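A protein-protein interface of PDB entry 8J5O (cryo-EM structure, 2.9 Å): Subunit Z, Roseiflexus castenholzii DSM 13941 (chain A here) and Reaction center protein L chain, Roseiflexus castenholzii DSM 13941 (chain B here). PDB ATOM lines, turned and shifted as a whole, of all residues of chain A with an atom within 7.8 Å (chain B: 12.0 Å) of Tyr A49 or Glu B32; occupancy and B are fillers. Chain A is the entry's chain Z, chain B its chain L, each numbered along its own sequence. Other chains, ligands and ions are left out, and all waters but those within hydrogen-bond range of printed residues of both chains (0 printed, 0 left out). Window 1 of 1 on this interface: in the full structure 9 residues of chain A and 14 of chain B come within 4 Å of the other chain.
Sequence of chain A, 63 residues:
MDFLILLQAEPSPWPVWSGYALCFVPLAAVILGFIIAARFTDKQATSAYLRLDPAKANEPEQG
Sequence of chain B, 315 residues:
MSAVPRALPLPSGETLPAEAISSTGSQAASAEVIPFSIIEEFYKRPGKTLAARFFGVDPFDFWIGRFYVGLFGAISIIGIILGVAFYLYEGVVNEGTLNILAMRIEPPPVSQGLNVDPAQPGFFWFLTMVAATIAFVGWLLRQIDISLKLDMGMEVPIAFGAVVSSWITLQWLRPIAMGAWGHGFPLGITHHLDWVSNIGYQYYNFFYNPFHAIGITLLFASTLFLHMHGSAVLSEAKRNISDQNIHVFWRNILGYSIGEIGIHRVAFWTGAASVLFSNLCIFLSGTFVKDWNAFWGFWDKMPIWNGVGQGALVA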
ATOM      1  N   LYS A  43      21.218  -5.082 -30.065  1.00  0.00           N
ATOM      2  CA  LYS A  43      22.486  -5.153 -29.339  1.00  0.00           C
ATOM      3  C   LYS A  43      22.354  -5.982 -28.069  1.00  0.00           C
ATOM      4  O   LYS A  43      23.203  -6.835 -27.781  1.00  0.00           O
ATOM      5  CB  LYS A  43      22.990  -3.753 -28.989  1.00  0.00           C
ATOM      6  CG  LYS A  43      24.369  -3.782 -28.338  1.00  0.00           C
ATOM      7  CD  LYS A  43      24.870  -2.411 -27.911  1.00  0.00           C
ATOM      8  CE  LYS A  43      25.297  -1.572 -29.086  1.00  0.00           C
ATOM      9  NZ  LYS A  43      25.899  -0.277 -28.672  1.00  0.00           N
ATOM     10  N   GLN A  44      21.300  -5.739 -27.288  1.00  0.00           N
ATOM     11  CA  GLN A  44      21.112  -6.512 -26.063  1.00  0.00           C
ATOM     12  C   GLN A  44      20.818  -7.974 -26.375  1.00  0.00           C
ATOM     13  O   GLN A  44      21.285  -8.871 -25.666  1.00  0.00           O
ATOM     14  CB  GLN A  44      19.992  -5.906 -25.218  1.00  0.00           C
ATOM     15  CG  GLN A  44      19.601  -6.749 -24.012  1.00  0.00           C
ATOM     16  CD  GLN A  44      20.789  -7.137 -23.156  1.00  0.00           C
ATOM     17  OE1 GLN A  44      21.742  -6.373 -23.012  1.00  0.00           O
ATOM     18  NE2 GLN A  44      20.739  -8.331 -22.581  1.00  0.00           N
ATOM     19  N   ALA A  45      20.044  -8.233 -27.432  1.00  0.00           N
ATOM     20  CA  ALA A  45      19.671  -9.605 -27.762  1.00  0.00           C
ATOM     21  C   ALA A  45      20.877 -10.431 -28.190  1.00  0.00           C
ATOM     22  O   ALA A  45      21.007 -11.597 -27.803  1.00  0.00           O
ATOM     23  CB  ALA A  45      18.607  -9.607 -28.858  1.00  0.00           C
ATOM     24  N   THR A  46      21.771  -9.849 -28.992  1.00  0.00           N
ATOM     25  CA  THR A  46      22.885 -10.619 -29.536  1.00  0.00           C
ATOM     26  C   THR A  46      24.104 -10.656 -28.621  1.00  0.00           C
ATOM     27  O   THR A  46      25.121 -11.244 -29.001  1.00  0.00           O
ATOM     28  CB  THR A  46      23.293 -10.068 -30.904  1.00  0.00           C
ATOM     29  OG1 THR A  46      23.722  -8.709 -30.770  1.00  0.00           O
ATOM     30  CG2 THR A  46      22.128 -10.137 -31.874  1.00  0.00           C
ATOM     31  N   SER A  47      24.033 -10.051 -27.439  1.00  0.00           N
ATOM     32  CA  SER A  47      25.157 -10.092 -26.514  1.00  0.00           C
ATOM     33  C   SER A  47      25.370 -11.509 -25.986  1.00  0.00           C
ATOM     34  O   SER A  47      24.620 -12.439 -26.294  1.00  0.00           O
ATOM     35  CB  SER A  47      24.928  -9.129 -25.351  1.00  0.00           C
ATOM     36  OG  SER A  47      23.686  -9.383 -24.722  1.00  0.00           O
ATOM     37  N   ALA A  48      26.416 -11.667 -25.179  1.00  0.00           N
ATOM     38  CA  ALA A  48      26.762 -12.949 -24.583  1.00  0.00           C
ATOM     39  C   ALA A  48      26.291 -12.995 -23.135  1.00  0.00           C
ATOM     40  O   ALA A  48      26.621 -12.109 -22.341  1.00  0.00           O
ATOM     41  CB  ALA A  48      28.269 -13.196 -24.654  1.00  0.00           C
ATOM     42  N   TYR A  49      25.526 -14.027 -22.797  1.00  0.00           N
ATOM     43  CA  TYR A  49      25.043 -14.228 -21.436  1.00  0.00           C
ATOM     44  C   TYR A  49      24.771 -15.716 -21.241  1.00  0.00           C
ATOM     45  O   TYR A  49      25.109 -16.541 -22.097  1.00  0.00           O
ATOM     46  CB  TYR A  49      23.818 -13.349 -21.156  1.00  0.00           C
ATOM     47  CG  TYR A  49      22.727 -13.392 -22.206  1.00  0.00           C
ATOM     48  CD1 TYR A  49      21.924 -14.512 -22.365  1.00  0.00           C
ATOM     49  CD2 TYR A  49      22.492 -12.301 -23.030  1.00  0.00           C
ATOM     50  CE1 TYR A  49      20.928 -14.546 -23.317  1.00  0.00           C
ATOM     51  CE2 TYR A  49      21.500 -12.329 -23.985  1.00  0.00           C
ATOM     52  CZ  TYR A  49      20.720 -13.454 -24.124  1.00  0.00           C
ATOM     53  OH  TYR A  49      19.729 -13.485 -25.075  1.00  0.00           O
ATOM     54  N   LEU A  50      24.162 -16.064 -20.107  1.00  0.00           N
ATOM     55  CA  LEU A  50      23.908 -17.466 -19.798  1.00  0.00           C
ATOM     56  C   LEU A  50      22.951 -18.095 -20.802  1.00  0.00           C
ATOM     57  O   LEU A  50      21.925 -17.512 -21.164  1.00  0.00           O
ATOM     58  CB  LEU A  50      23.343 -17.617 -18.384  1.00  0.00           C
ATOM     59  CG  LEU A  50      24.300 -17.522 -17.195  1.00  0.00           C
ATOM     60  CD1 LEU A  50      24.792 -16.110 -16.977  1.00  0.00           C
ATOM     61  CD2 LEU A  50      23.625 -18.055 -15.943  1.00  0.00           C
ATOM     62  N   ARG A  51      23.296 -19.300 -21.246  1.00  0.00           N
ATOM     63  CA  ARG A  51      22.460 -20.071 -22.153  1.00  0.00           C
ATOM     64  C   ARG A  51      22.699 -21.548 -21.887  1.00  0.00           C
ATOM     65  O   ARG A  51      23.730 -21.940 -21.335  1.00  0.00           O
ATOM     66  CB  ARG A  51      22.753 -19.741 -23.621  1.00  0.00           C
ATOM     67  CG  ARG A  51      22.159 -18.434 -24.113  1.00  0.00           C
ATOM     68  CD  ARG A  51      23.054 -17.785 -25.157  1.00  0.00           C
ATOM     69  NE  ARG A  51      22.390 -16.703 -25.871  1.00  0.00           N
ATOM     70  CZ  ARG A  51      22.956 -15.538 -26.158  1.00  0.00           C
ATOM     71  NH1 ARG A  51      24.195 -15.262 -25.791  1.00  0.00           N
ATOM     72  NH2 ARG A  51      22.259 -14.624 -26.828  1.00  0.00           N
ATOM     73  N   LEU A  52      21.733 -22.368 -22.286  1.00  0.00           N
ATOM     74  CA  LEU A  52      21.874 -23.815 -22.207  1.00  0.00           C
ATOM     75  C   LEU A  52      22.531 -24.321 -23.484  1.00  0.00           C
ATOM     76  O   LEU A  52      22.180 -23.883 -24.584  1.00  0.00           O
ATOM     77  CB  LEU A  52      20.516 -24.484 -22.000  1.00  0.00           C
ATOM     78  CG  LEU A  52      19.820 -24.189 -20.669  1.00  0.00           C
ATOM     79  CD1 LEU A  52      18.429 -24.794 -20.644  1.00  0.00           C
ATOM     80  CD2 LEU A  52      20.649 -24.701 -19.502  1.00  0.00           C
ATOM     81  N   ASP A  53      23.484 -25.230 -23.335  1.00  0.00           N
ATOM     82  CA  ASP A  53      24.250 -25.715 -24.473  1.00  0.00           C
ATOM     83  C   ASP A  53      23.344 -26.476 -25.434  1.00  0.00           C
ATOM     84  O   ASP A  53      22.693 -27.446 -25.020  1.00  0.00           O
ATOM     85  CB  ASP A  53      25.390 -26.608 -23.990  1.00  0.00           C
ATOM     86  CG  ASP A  53      26.313 -27.034 -25.112  1.00  0.00           C
ATOM     87  OD1 ASP A  53      27.108 -26.193 -25.581  1.00  0.00           O
ATOM     88  OD2 ASP A  53      26.248 -28.211 -25.519  1.00  0.00           O
ATOM     89  N   PRO A  54      23.260 -26.072 -26.705  1.00  0.00           N
ATOM     90  CA  PRO A  54      22.380 -26.788 -27.644  1.00  0.00           C
ATOM     91  C   PRO A  54      22.776 -28.236 -27.866  1.00  0.00           C
ATOM     92  O   PRO A  54      21.905 -29.071 -28.139  1.00  0.00           O
ATOM     93  CB  PRO A  54      22.497 -25.963 -28.934  1.00  0.00           C
ATOM     94  CG  PRO A  54      23.770 -25.199 -28.792  1.00  0.00           C
ATOM     95  CD  PRO A  54      23.921 -24.917 -27.333  1.00  0.00           C
ATOM     96  N   LYS A  56      24.013 -30.405 -25.605  1.00  0.00           N
ATOM     97  CA  LYS A  56      23.436 -31.185 -24.516  1.00  0.00           C
ATOM     98  C   LYS A  56      21.923 -31.017 -24.450  1.00  0.00           C
ATOM     99  O   LYS A  56      21.199 -31.971 -24.141  1.00  0.00           O
ATOM    100  CB  LYS A  56      24.083 -30.793 -23.187  1.00  0.00           C
ATOM    101  CG  LYS A  56      23.760 -29.384 -22.719  1.00  0.00           C
ATOM    102  CD  LYS A  56      24.455 -29.062 -21.405  1.00  0.00           C
ATOM    103  CE  LYS A  56      24.164 -27.636 -20.960  1.00  0.00           C
ATOM    104  NZ  LYS A  56      22.734 -27.446 -20.604  1.00  0.00           N
ATOM    105  N   ALA B   7      31.571 -12.659 -12.750  1.00  0.00           N
ATOM    106  CA  ALA B   7      30.131 -12.444 -12.660  1.00  0.00           C
ATOM    107  C   ALA B   7      29.426 -12.922 -13.925  1.00  0.00           C
ATOM    108  O   ALA B   7      29.911 -12.712 -15.036  1.00  0.00           O
ATOM    109  CB  ALA B   7      29.830 -10.978 -12.408  1.00  0.00           C
ATOM    110  N   LEU B   8      28.276 -13.567 -13.745  1.00  0.00           N
ATOM    111  CA  LEU B   8      27.524 -14.125 -14.861  1.00  0.00           C
ATOM    112  C   LEU B   8      26.486 -13.120 -15.341  1.00  0.00           C
ATOM    113  O   LEU B   8      25.622 -12.717 -14.550  1.00  0.00           O
ATOM    114  CB  LEU B   8      26.844 -15.420 -14.449  1.00  0.00           C
ATOM    115  CG  LEU B   8      27.750 -16.462 -13.793  1.00  0.00           C
ATOM    116  CD1 LEU B   8      27.045 -17.804 -13.695  1.00  0.00           C
ATOM    117  CD2 LEU B   8      29.054 -16.591 -14.566  1.00  0.00           C
ATOM    118  N   PRO B   9      26.529 -12.688 -16.602  1.00  0.00           N
ATOM    119  CA  PRO B   9      25.510 -11.754 -17.102  1.00  0.00           C
ATOM    120  C   PRO B   9      24.224 -12.488 -17.455  1.00  0.00           C
ATOM    121  O   PRO B   9      24.240 -13.475 -18.192  1.00  0.00           O
ATOM    122  CB  PRO B   9      26.163 -11.141 -18.350  1.00  0.00           C
ATOM    123  CG  PRO B   9      27.563 -11.715 -18.418  1.00  0.00           C
ATOM    124  CD  PRO B   9      27.561 -12.966 -17.609  1.00  0.00           C
ATOM    125  N   LEU B  10      23.109 -11.998 -16.928  1.00  0.00           N
ATOM    126  CA  LEU B  10      21.810 -12.598 -17.190  1.00  0.00           C
ATOM    127  C   LEU B  10      21.192 -12.019 -18.456  1.00  0.00           C
ATOM    128  O   LEU B  10      21.577 -10.939 -18.913  1.00  0.00           O
ATOM    129  CB  LEU B  10      20.879 -12.372 -16.001  1.00  0.00           C
ATOM    130  CG  LEU B  10      20.924 -13.435 -14.901  1.00  0.00           C
ATOM    131  CD1 LEU B  10      22.281 -13.452 -14.220  1.00  0.00           C
ATOM    132  CD2 LEU B  10      19.817 -13.203 -13.885  1.00  0.00           C
ATOM    133  N   PRO B  11      20.239 -12.737 -19.059  1.00  0.00           N
ATOM    134  CA  PRO B  11      19.582 -12.208 -20.267  1.00  0.00           C
ATOM    135  C   PRO B  11      18.886 -10.877 -20.051  1.00  0.00           C
ATOM    136  O   PRO B  11      18.852 -10.047 -20.967  1.00  0.00           O
ATOM    137  CB  PRO B  11      18.585 -13.317 -20.629  1.00  0.00           C
ATOM    138  CG  PRO B  11      19.159 -14.550 -20.030  1.00  0.00           C
ATOM    139  CD  PRO B  11      19.833 -14.119 -18.765  1.00  0.00           C
ATOM    140  N   SER B  12      18.316 -10.649 -18.865  1.00  0.00           N
ATOM    141  CA  SER B  12      17.675  -9.367 -18.593  1.00  0.00           C
ATOM    142  C   SER B  12      18.689  -8.230 -18.601  1.00  0.00           C
ATOM    143  O   SER B  12      18.417  -7.148 -19.133  1.00  0.00           O
ATOM    144  CB  SER B  12      16.939  -9.421 -17.255  1.00  0.00           C
ATOM    145  OG  SER B  12      17.738 -10.035 -16.260  1.00  0.00           O
ATOM    146  N   GLY B  13      19.862  -8.457 -18.021  1.00  0.00           N
ATOM    147  CA  GLY B  13      20.889  -7.438 -17.954  1.00  0.00           C
ATOM    148  C   GLY B  13      21.588  -7.425 -16.612  1.00  0.00           C
ATOM    149  O   GLY B  13      22.548  -6.679 -16.405  1.00  0.00           O
ATOM    150  N   GLU B  14      21.107  -8.254 -15.691  1.00  0.00           N
ATOM    151  CA  GLU B  14      21.697  -8.330 -14.365  1.00  0.00           C
ATOM    152  C   GLU B  14      23.105  -8.912 -14.426  1.00  0.00           C
ATOM    153  O   GLU B  14      23.455  -9.664 -15.338  1.00  0.00           O
ATOM    154  CB  GLU B  14      20.832  -9.184 -13.441  1.00  0.00           C
ATOM    155  CG  GLU B  14      19.481  -8.582 -13.116  1.00  0.00           C
ATOM    156  CD  GLU B  14      18.656  -9.476 -12.214  1.00  0.00           C
ATOM    157  OE1 GLU B  14      19.088 -10.617 -11.948  1.00  0.00           O
ATOM    158  OE2 GLU B  14      17.579  -9.036 -11.765  1.00  0.00           O
ATOM    159  N   THR B  15      23.915  -8.544 -13.438  1.00  0.00           N
ATOM    160  CA  THR B  15      25.254  -9.093 -13.245  1.00  0.00           C
ATOM    161  C   THR B  15      25.256  -9.760 -11.872  1.00  0.00           C
ATOM    162  O   THR B  15      25.615  -9.142 -10.868  1.00  0.00           O
ATOM    163  CB  THR B  15      26.325  -8.008 -13.354  1.00  0.00           C
ATOM    164  OG1 THR B  15      26.269  -7.408 -14.654  1.00  0.00           O
ATOM    165  CG2 THR B  15      27.702  -8.599 -13.138  1.00  0.00           C
ATOM    166  N   LEU B  16      24.849 -11.029 -11.836  1.00  0.00           N
ATOM    167  CA  LEU B  16      24.683 -11.751 -10.584  1.00  0.00           C
ATOM    168  C   LEU B  16      25.885 -12.645 -10.336  1.00  0.00           C
ATOM    169  O   LEU B  16      26.168 -13.524 -11.166  1.00  0.00           O
ATOM    170  CB  LEU B  16      23.409 -12.587 -10.616  1.00  0.00           C
ATOM    171  CG  LEU B  16      22.087 -11.846 -10.424  1.00  0.00           C
ATOM    172  CD1 LEU B  16      20.976 -12.828 -10.087  1.00  0.00           C
ATOM    173  CD2 LEU B  16      22.213 -10.780  -9.348  1.00  0.00           C
ATOM    174  N   ALA B  18      27.910 -15.797  -9.152  1.00  0.00           N
ATOM    175  CA  ALA B  18      27.487 -17.188  -9.058  1.00  0.00           C
ATOM    176  C   ALA B  18      27.492 -17.670  -7.612  1.00  0.00           C
ATOM    177  O   ALA B  18      26.788 -18.617  -7.263  1.00  0.00           O
ATOM    178  CB  ALA B  18      28.382 -18.073  -9.914  1.00  0.00           C
ATOM    179  N   ALA B  29      22.843 -24.705 -11.543  1.00  0.00           N
ATOM    180  CA  ALA B  29      22.260 -24.815 -12.873  1.00  0.00           C
ATOM    181  C   ALA B  29      23.297 -25.289 -13.884  1.00  0.00           C
ATOM    182  O   ALA B  29      24.491 -25.344 -13.584  1.00  0.00           O
ATOM    183  CB  ALA B  29      21.669 -23.481 -13.306  1.00  0.00           C
ATOM    184  N   SER B  30      22.834 -25.634 -15.085  1.00  0.00           N
ATOM    185  CA  SER B  30      23.705 -26.062 -16.170  1.00  0.00           C
ATOM    186  C   SER B  30      23.932 -24.960 -17.198  1.00  0.00           C
ATOM    187  O   SER B  30      24.447 -25.230 -18.288  1.00  0.00           O
ATOM    188  CB  SER B  30      23.133 -27.309 -16.847  1.00  0.00           C
ATOM    189  OG  SER B  30      23.951 -27.723 -17.927  1.00  0.00           O
ATOM    190  N   ALA B  31      23.555 -23.727 -16.876  1.00  0.00           N
ATOM    191  CA  ALA B  31      23.736 -22.616 -17.794  1.00  0.00           C
ATOM    192  C   ALA B  31      25.202 -22.198 -17.852  1.00  0.00           C
ATOM    193  O   ALA B  31      26.012 -22.544 -16.989  1.00  0.00           O
ATOM    194  CB  ALA B  31      22.864 -21.430 -17.381  1.00  0.00           C
ATOM    195  N   GLU B  32      25.536 -21.445 -18.896  1.00  0.00           N
ATOM    196  CA  GLU B  32      26.895 -20.962 -19.091  1.00  0.00           C
ATOM    197  C   GLU B  32      26.860 -19.789 -20.059  1.00  0.00           C
ATOM    198  O   GLU B  32      25.877 -19.582 -20.775  1.00  0.00           O
ATOM    199  CB  GLU B  32      27.811 -22.074 -19.607  1.00  0.00           C
ATOM    200  CG  GLU B  32      27.456 -22.577 -20.994  1.00  0.00           C
ATOM    201  CD  GLU B  32      28.343 -23.722 -21.442  1.00  0.00           C
ATOM    202  OE1 GLU B  32      29.219 -24.138 -20.656  1.00  0.00           O
ATOM    203  OE2 GLU B  32      28.164 -24.205 -22.579  1.00  0.00           O
ATOM    204  N   VAL B  33      27.948 -19.024 -20.072  1.00  0.00           N
ATOM    205  CA  VAL B  33      28.052 -17.853 -20.938  1.00  0.00           C
ATOM    206  C   VAL B  33      28.467 -18.325 -22.327  1.00  0.00           C
ATOM    207  O   VAL B  33      29.606 -18.748 -22.536  1.00  0.00           O
ATOM    208  CB  VAL B  33      29.043 -16.826 -20.380  1.00  0.00           C
ATOM    209  CG1 VAL B  33      29.210 -15.672 -21.353  1.00  0.00           C
ATOM    210  CG2 VAL B  33      28.568 -16.319 -19.030  1.00  0.00           C
ATOM    211  N   ILE B  34      27.543 -18.246 -23.280  1.00  0.00           N
ATOM    212  CA  ILE B  34      27.746 -18.741 -24.634  1.00  0.00           C
ATOM    213  C   ILE B  34      27.513 -17.586 -25.598  1.00  0.00           C
ATOM    214  O   ILE B  34      26.466 -16.941 -25.530  1.00  0.00           O
ATOM    215  CB  ILE B  34      26.811 -19.915 -24.977  1.00  0.00           C
ATOM    216  CG1 ILE B  34      27.100 -21.110 -24.069  1.00  0.00           C
ATOM    217  CG2 ILE B  34      26.960 -20.305 -26.435  1.00  0.00           C
ATOM    218  CD1 ILE B  34      26.064 -22.207 -24.161  1.00  0.00           C
ATOM    219  N   PRO B  35      28.448 -17.288 -26.497  1.00  0.00           N
ATOM    220  CA  PRO B  35      28.188 -16.269 -27.518  1.00  0.00           C
ATOM    221  C   PRO B  35      27.122 -16.724 -28.503  1.00  0.00           C
ATOM    222  O   PRO B  35      26.891 -17.918 -28.702  1.00  0.00           O
ATOM    223  CB  PRO B  35      29.547 -16.100 -28.209  1.00  0.00           C
ATOM    224  CG  PRO B  35      30.281 -17.364 -27.923  1.00  0.00           C
ATOM    225  CD  PRO B  35      29.821 -17.815 -26.571  1.00  0.00           C
ATOM    226  N   PHE B  36      26.466 -15.741 -29.126  1.00  0.00           N
ATOM    227  CA  PHE B  36      25.409 -16.030 -30.091  1.00  0.00           C
ATOM    228  C   PHE B  36      25.930 -16.741 -31.335  1.00  0.00           C
ATOM    229  O   PHE B  36      25.140 -17.360 -32.057  1.00  0.00           O
ATOM    230  CB  PHE B  36      24.705 -14.733 -30.492  1.00  0.00           C
ATOM    231  CG  PHE B  36      23.355 -14.941 -31.117  1.00  0.00           C
ATOM    232  CD1 PHE B  36      22.230 -15.099 -30.330  1.00  0.00           C
ATOM    233  CD2 PHE B  36      23.213 -14.981 -32.492  1.00  0.00           C
ATOM    234  CE1 PHE B  36      20.990 -15.290 -30.902  1.00  0.00           C
ATOM    235  CE2 PHE B  36      21.975 -15.173 -33.067  1.00  0.00           C
ATOM    236  CZ  PHE B  36      20.863 -15.327 -32.272  1.00  0.00           C
ATOM    237  N   SER B  37      27.236 -16.663 -31.600  1.00  0.00           N
ATOM    238  CA  SER B  37      27.799 -17.279 -32.796  1.00  0.00           C
ATOM    239  C   SER B  37      27.633 -18.794 -32.776  1.00  0.00           C
ATOM    240  O   SER B  37      27.330 -19.408 -33.806  1.00  0.00           O
ATOM    241  CB  SER B  37      29.274 -16.904 -32.923  1.00  0.00           C
ATOM    242  OG  SER B  37      29.422 -15.507 -33.110  1.00  0.00           O
ATOM    243  N   ILE B  38      27.838 -19.416 -31.612  1.00  0.00           N
ATOM    244  CA  ILE B  38      27.711 -20.867 -31.503  1.00  0.00           C
ATOM    245  C   ILE B  38      26.281 -21.301 -31.797  1.00  0.00           C
ATOM    246  O   ILE B  38      26.044 -22.260 -32.542  1.00  0.00           O
ATOM    247  CB  ILE B  38      28.168 -21.341 -30.111  1.00  0.00           C
ATOM    248  CG1 ILE B  38      29.623 -20.938 -29.861  1.00  0.00           C
ATOM    249  CG2 ILE B  38      27.994 -22.842 -29.973  1.00  0.00           C
ATOM    250  CD1 ILE B  38      30.599 -21.543 -30.844  1.00  0.00           C
ATOM    251  N   ILE B  39      25.306 -20.598 -31.217  1.00  0.00           N
ATOM    252  CA  ILE B  39      23.904 -20.925 -31.463  1.00  0.00           C
ATOM    253  C   ILE B  39      23.561 -20.726 -32.932  1.00  0.00           C
ATOM    254  O   ILE B  39      22.865 -21.549 -33.538  1.00  0.00           O
ATOM    255  CB  ILE B  39      22.985 -20.091 -30.551  1.00  0.00           C
ATOM    256  CG1 ILE B  39      23.238 -20.417 -29.076  1.00  0.00           C
ATOM    257  CG2 ILE B  39      21.529 -20.323 -30.907  1.00  0.00           C
ATOM    258  CD1 ILE B  39      24.313 -19.578 -28.432  1.00  0.00           C
ATOM    259  N   GLU B  40      24.040 -19.632 -33.528  1.00  0.00           N
ATOM    260  CA  GLU B  40      23.736 -19.361 -34.930  1.00  0.00           C
ATOM    261  C   GLU B  40      24.311 -20.441 -35.840  1.00  0.00           C
ATOM    262  O   GLU B  40      23.658 -20.866 -36.800  1.00  0.00           O
ATOM    263  CB  GLU B  40      24.269 -17.984 -35.321  1.00  0.00           C
ATOM    264  CG  GLU B  40      24.370 -17.753 -36.818  1.00  0.00           C
ATOM    265  CD  GLU B  40      23.067 -17.264 -37.413  1.00  0.00           C
ATOM    266  OE1 GLU B  40      22.070 -17.187 -36.666  1.00  0.00           O
ATOM    267  OE2 GLU B  40      23.039 -16.951 -38.620  1.00  0.00           O
ATOM    268  N   PHE B  42      25.041 -23.589 -34.945  1.00  0.00           N
ATOM    269  CA  PHE B  42      24.540 -24.927 -34.637  1.00  0.00           C
ATOM    270  C   PHE B  42      23.245 -25.233 -35.384  1.00  0.00           C
ATOM    271  O   PHE B  42      23.042 -26.364 -35.840  1.00  0.00           O
ATOM    272  CB  PHE B  42      24.362 -25.068 -33.118  1.00  0.00           C
ATOM    273  CG  PHE B  42      23.818 -26.405 -32.670  1.00  0.00           C
ATOM    274  CD1 PHE B  42      22.453 -26.651 -32.619  1.00  0.00           C
ATOM    275  CD2 PHE B  42      24.684 -27.422 -32.307  1.00  0.00           C
ATOM    276  CE1 PHE B  42      21.969 -27.877 -32.208  1.00  0.00           C
ATOM    277  CE2 PHE B  42      24.204 -28.651 -31.899  1.00  0.00           C
ATOM    278  CZ  PHE B  42      22.846 -28.878 -31.851  1.00  0.00           C
ATOM    279  N   TYR B  43      22.361 -24.248 -35.521  1.00  0.00           N
ATOM    280  CA  TYR B  43      20.987 -24.485 -35.946  1.00  0.00           C
ATOM    281  C   TYR B  43      20.749 -24.259 -37.436  1.00  0.00           C
ATOM    282  O   TYR B  43      19.587 -24.160 -37.843  1.00  0.00           O
ATOM    283  CB  TYR B  43      20.029 -23.593 -35.155  1.00  0.00           C
ATOM    284  CG  TYR B  43      19.719 -24.064 -33.751  1.00  0.00           C
ATOM    285  CD1 TYR B  43      18.712 -24.988 -33.516  1.00  0.00           C
ATOM    286  CD2 TYR B  43      20.421 -23.570 -32.661  1.00  0.00           C
ATOM    287  CE1 TYR B  43      18.421 -25.416 -32.235  1.00  0.00           C
ATOM    288  CE2 TYR B  43      20.135 -23.990 -31.377  1.00  0.00           C
ATOM    289  CZ  TYR B  43      19.134 -24.914 -31.171  1.00  0.00           C
ATOM    290  OH  TYR B  43      18.847 -25.338 -29.896  1.00  0.00           O
ATOM    291  N   LYS B 238      13.238  -8.776 -12.113  1.00  0.00           N
ATOM    292  CA  LYS B 238      14.508  -8.613 -11.411  1.00  0.00           C
ATOM    293  C   LYS B 238      14.303  -8.642  -9.903  1.00  0.00           C
ATOM    294  O   LYS B 238      14.797  -7.788  -9.164  1.00  0.00           O
ATOM    295  CB  LYS B 238      15.176  -7.315 -11.852  1.00  0.00           C
ATOM    296  CG  LYS B 238      15.354  -7.214 -13.359  1.00  0.00           C
ATOM    297  CD  LYS B 238      15.981  -5.897 -13.766  1.00  0.00           C
ATOM    298  CE  LYS B 238      16.695  -6.027 -15.100  1.00  0.00           C
ATOM    299  NZ  LYS B 238      16.940  -4.702 -15.730  1.00  0.00           N
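The side-chain hydroxyl of Tyr A49 is in hydrogen-bond range of the guanidinium group of Arg A51 (3.3 Å).
N of Leu B16 lies within hydrogen-bond range of O of Leu B8 (3.3 Å).
OG of Ser A47 is in hydrogen-bond range of O of Gln A44.
The guanidinium group of Arg A51 sits at hydrogen-bond distance from the backbone carbonyl oxygen of Ser A47 (2.9 Å).
OD2 of Asp A53 is in hydrogen-bond range of N of Lys A56 (3.1 Å).
The side-chain amino group (NZ) of Lys A56 sits at hydrogen-bond distance from the side-chain hydroxyl (OG) of Ser B30, at 3.0 Å.
The backbone carbonyl oxygen (O) of Glu B32 sits at hydrogen-bond distance from the backbone NH (N) of Arg A51 (2.6 Å).
The backbone NH of Ile B34 is in hydrogen-bond range of the backbone carbonyl oxygen of Tyr A49 (3.2 Å).
O of Pro B11 is in hydrogen-bond range of NE2 of Gln A44 (3.0 Å).
The backbone carbonyl oxygen (O) of Tyr A49 sits close to the backbone carbonyl oxygen (O) of Glu B32 (3.4 Å).
The backbone carbonyl oxygen (O) of Pro B9 sits close to the backbone NH (N) of Leu A50, 3.2 Å away.
NH1 of Arg A51 lies within hydrogen-bond range of O of Ile B34, at 2.8 Å.
Printed residues of chain B that touch a printed residue of chain A: Leu B8, Pro B9, Leu B10, Pro B11, Ser B30, Ala B31, Glu B32, Val B33, Ile B34, Phe B36, Ile B39, Phe B42 and Tyr B43.
Hydrophobic or aromatic side chains of chain B that line the printed part of chain A: Leu B8, Pro B11, Ala B31, Ile B34, Phe B36, Ile B39, Phe B42 and Tyr B43.
Among the printed residues, no Asp or Glu carboxylate lies within 4 Å of a Lys or Arg side-chain nitrogen of the other chain.
Among the printed residues, pairs that only touch across the chains: Tyr A49 with Pro B9 (3.0 Å), Leu A50 with Glu B32 (3.1 Å), Leu A50 with Leu B8 (3.3 Å), Tyr A49 with Val B33 (3.4 Å), Arg A51 with Phe B36 (3.5 Å), Arg A51 with Ala B31 (3.6 Å), Tyr A49 with Pro B11 (3.6 Å), Leu A50 with Ala B31 (3.7 Å), Pro A54 with Phe B42 (3.7 Å), Asp A53 with Glu B32 (3.8 Å), Thr A46 with Phe B36 (3.8 Å), Pro A54 with Tyr B43 (3.8 Å), Arg A51 with Ile B39 (3.9 Å), Asp A53 with Ile B34 (3.96 Å) and Tyr A49 with Leu B10 (3.98 Å).
Lys A43 touches none of the printed residues of chain B.
Of chain B, only Pro B11 comes within 4 Å of Gln A44.
No residue of chain B comes within 4 Å of Ala A45.
Of the printed residues of chain B, Thr A46 touches Phe B36 (3.8 Å).
No residue of chain B comes within 4 Å of Ser A47.
Printed residues of chain B within 4 Å of Tyr A49: Pro B9 (3.0 Å), Leu B10 (3.98 Å), Pro B11 (3.6 Å), Glu B32 (3.4 Å), Val B33 (3.4 Å) and Ile B34 (3.2 Å).
Leu A50 touches just these residues of chain B: Leu B8, Pro B9, Ala B31 and Glu B32.
Printed residues of chain A within 4 Å of Leu B8: Leu A50.
Of the printed residues of chain A, Leu B10 touches Tyr A49.
Of chain A, only Tyr A49, Leu A50, Arg A51 and Asp A53 come within 4 Å of Glu B32.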
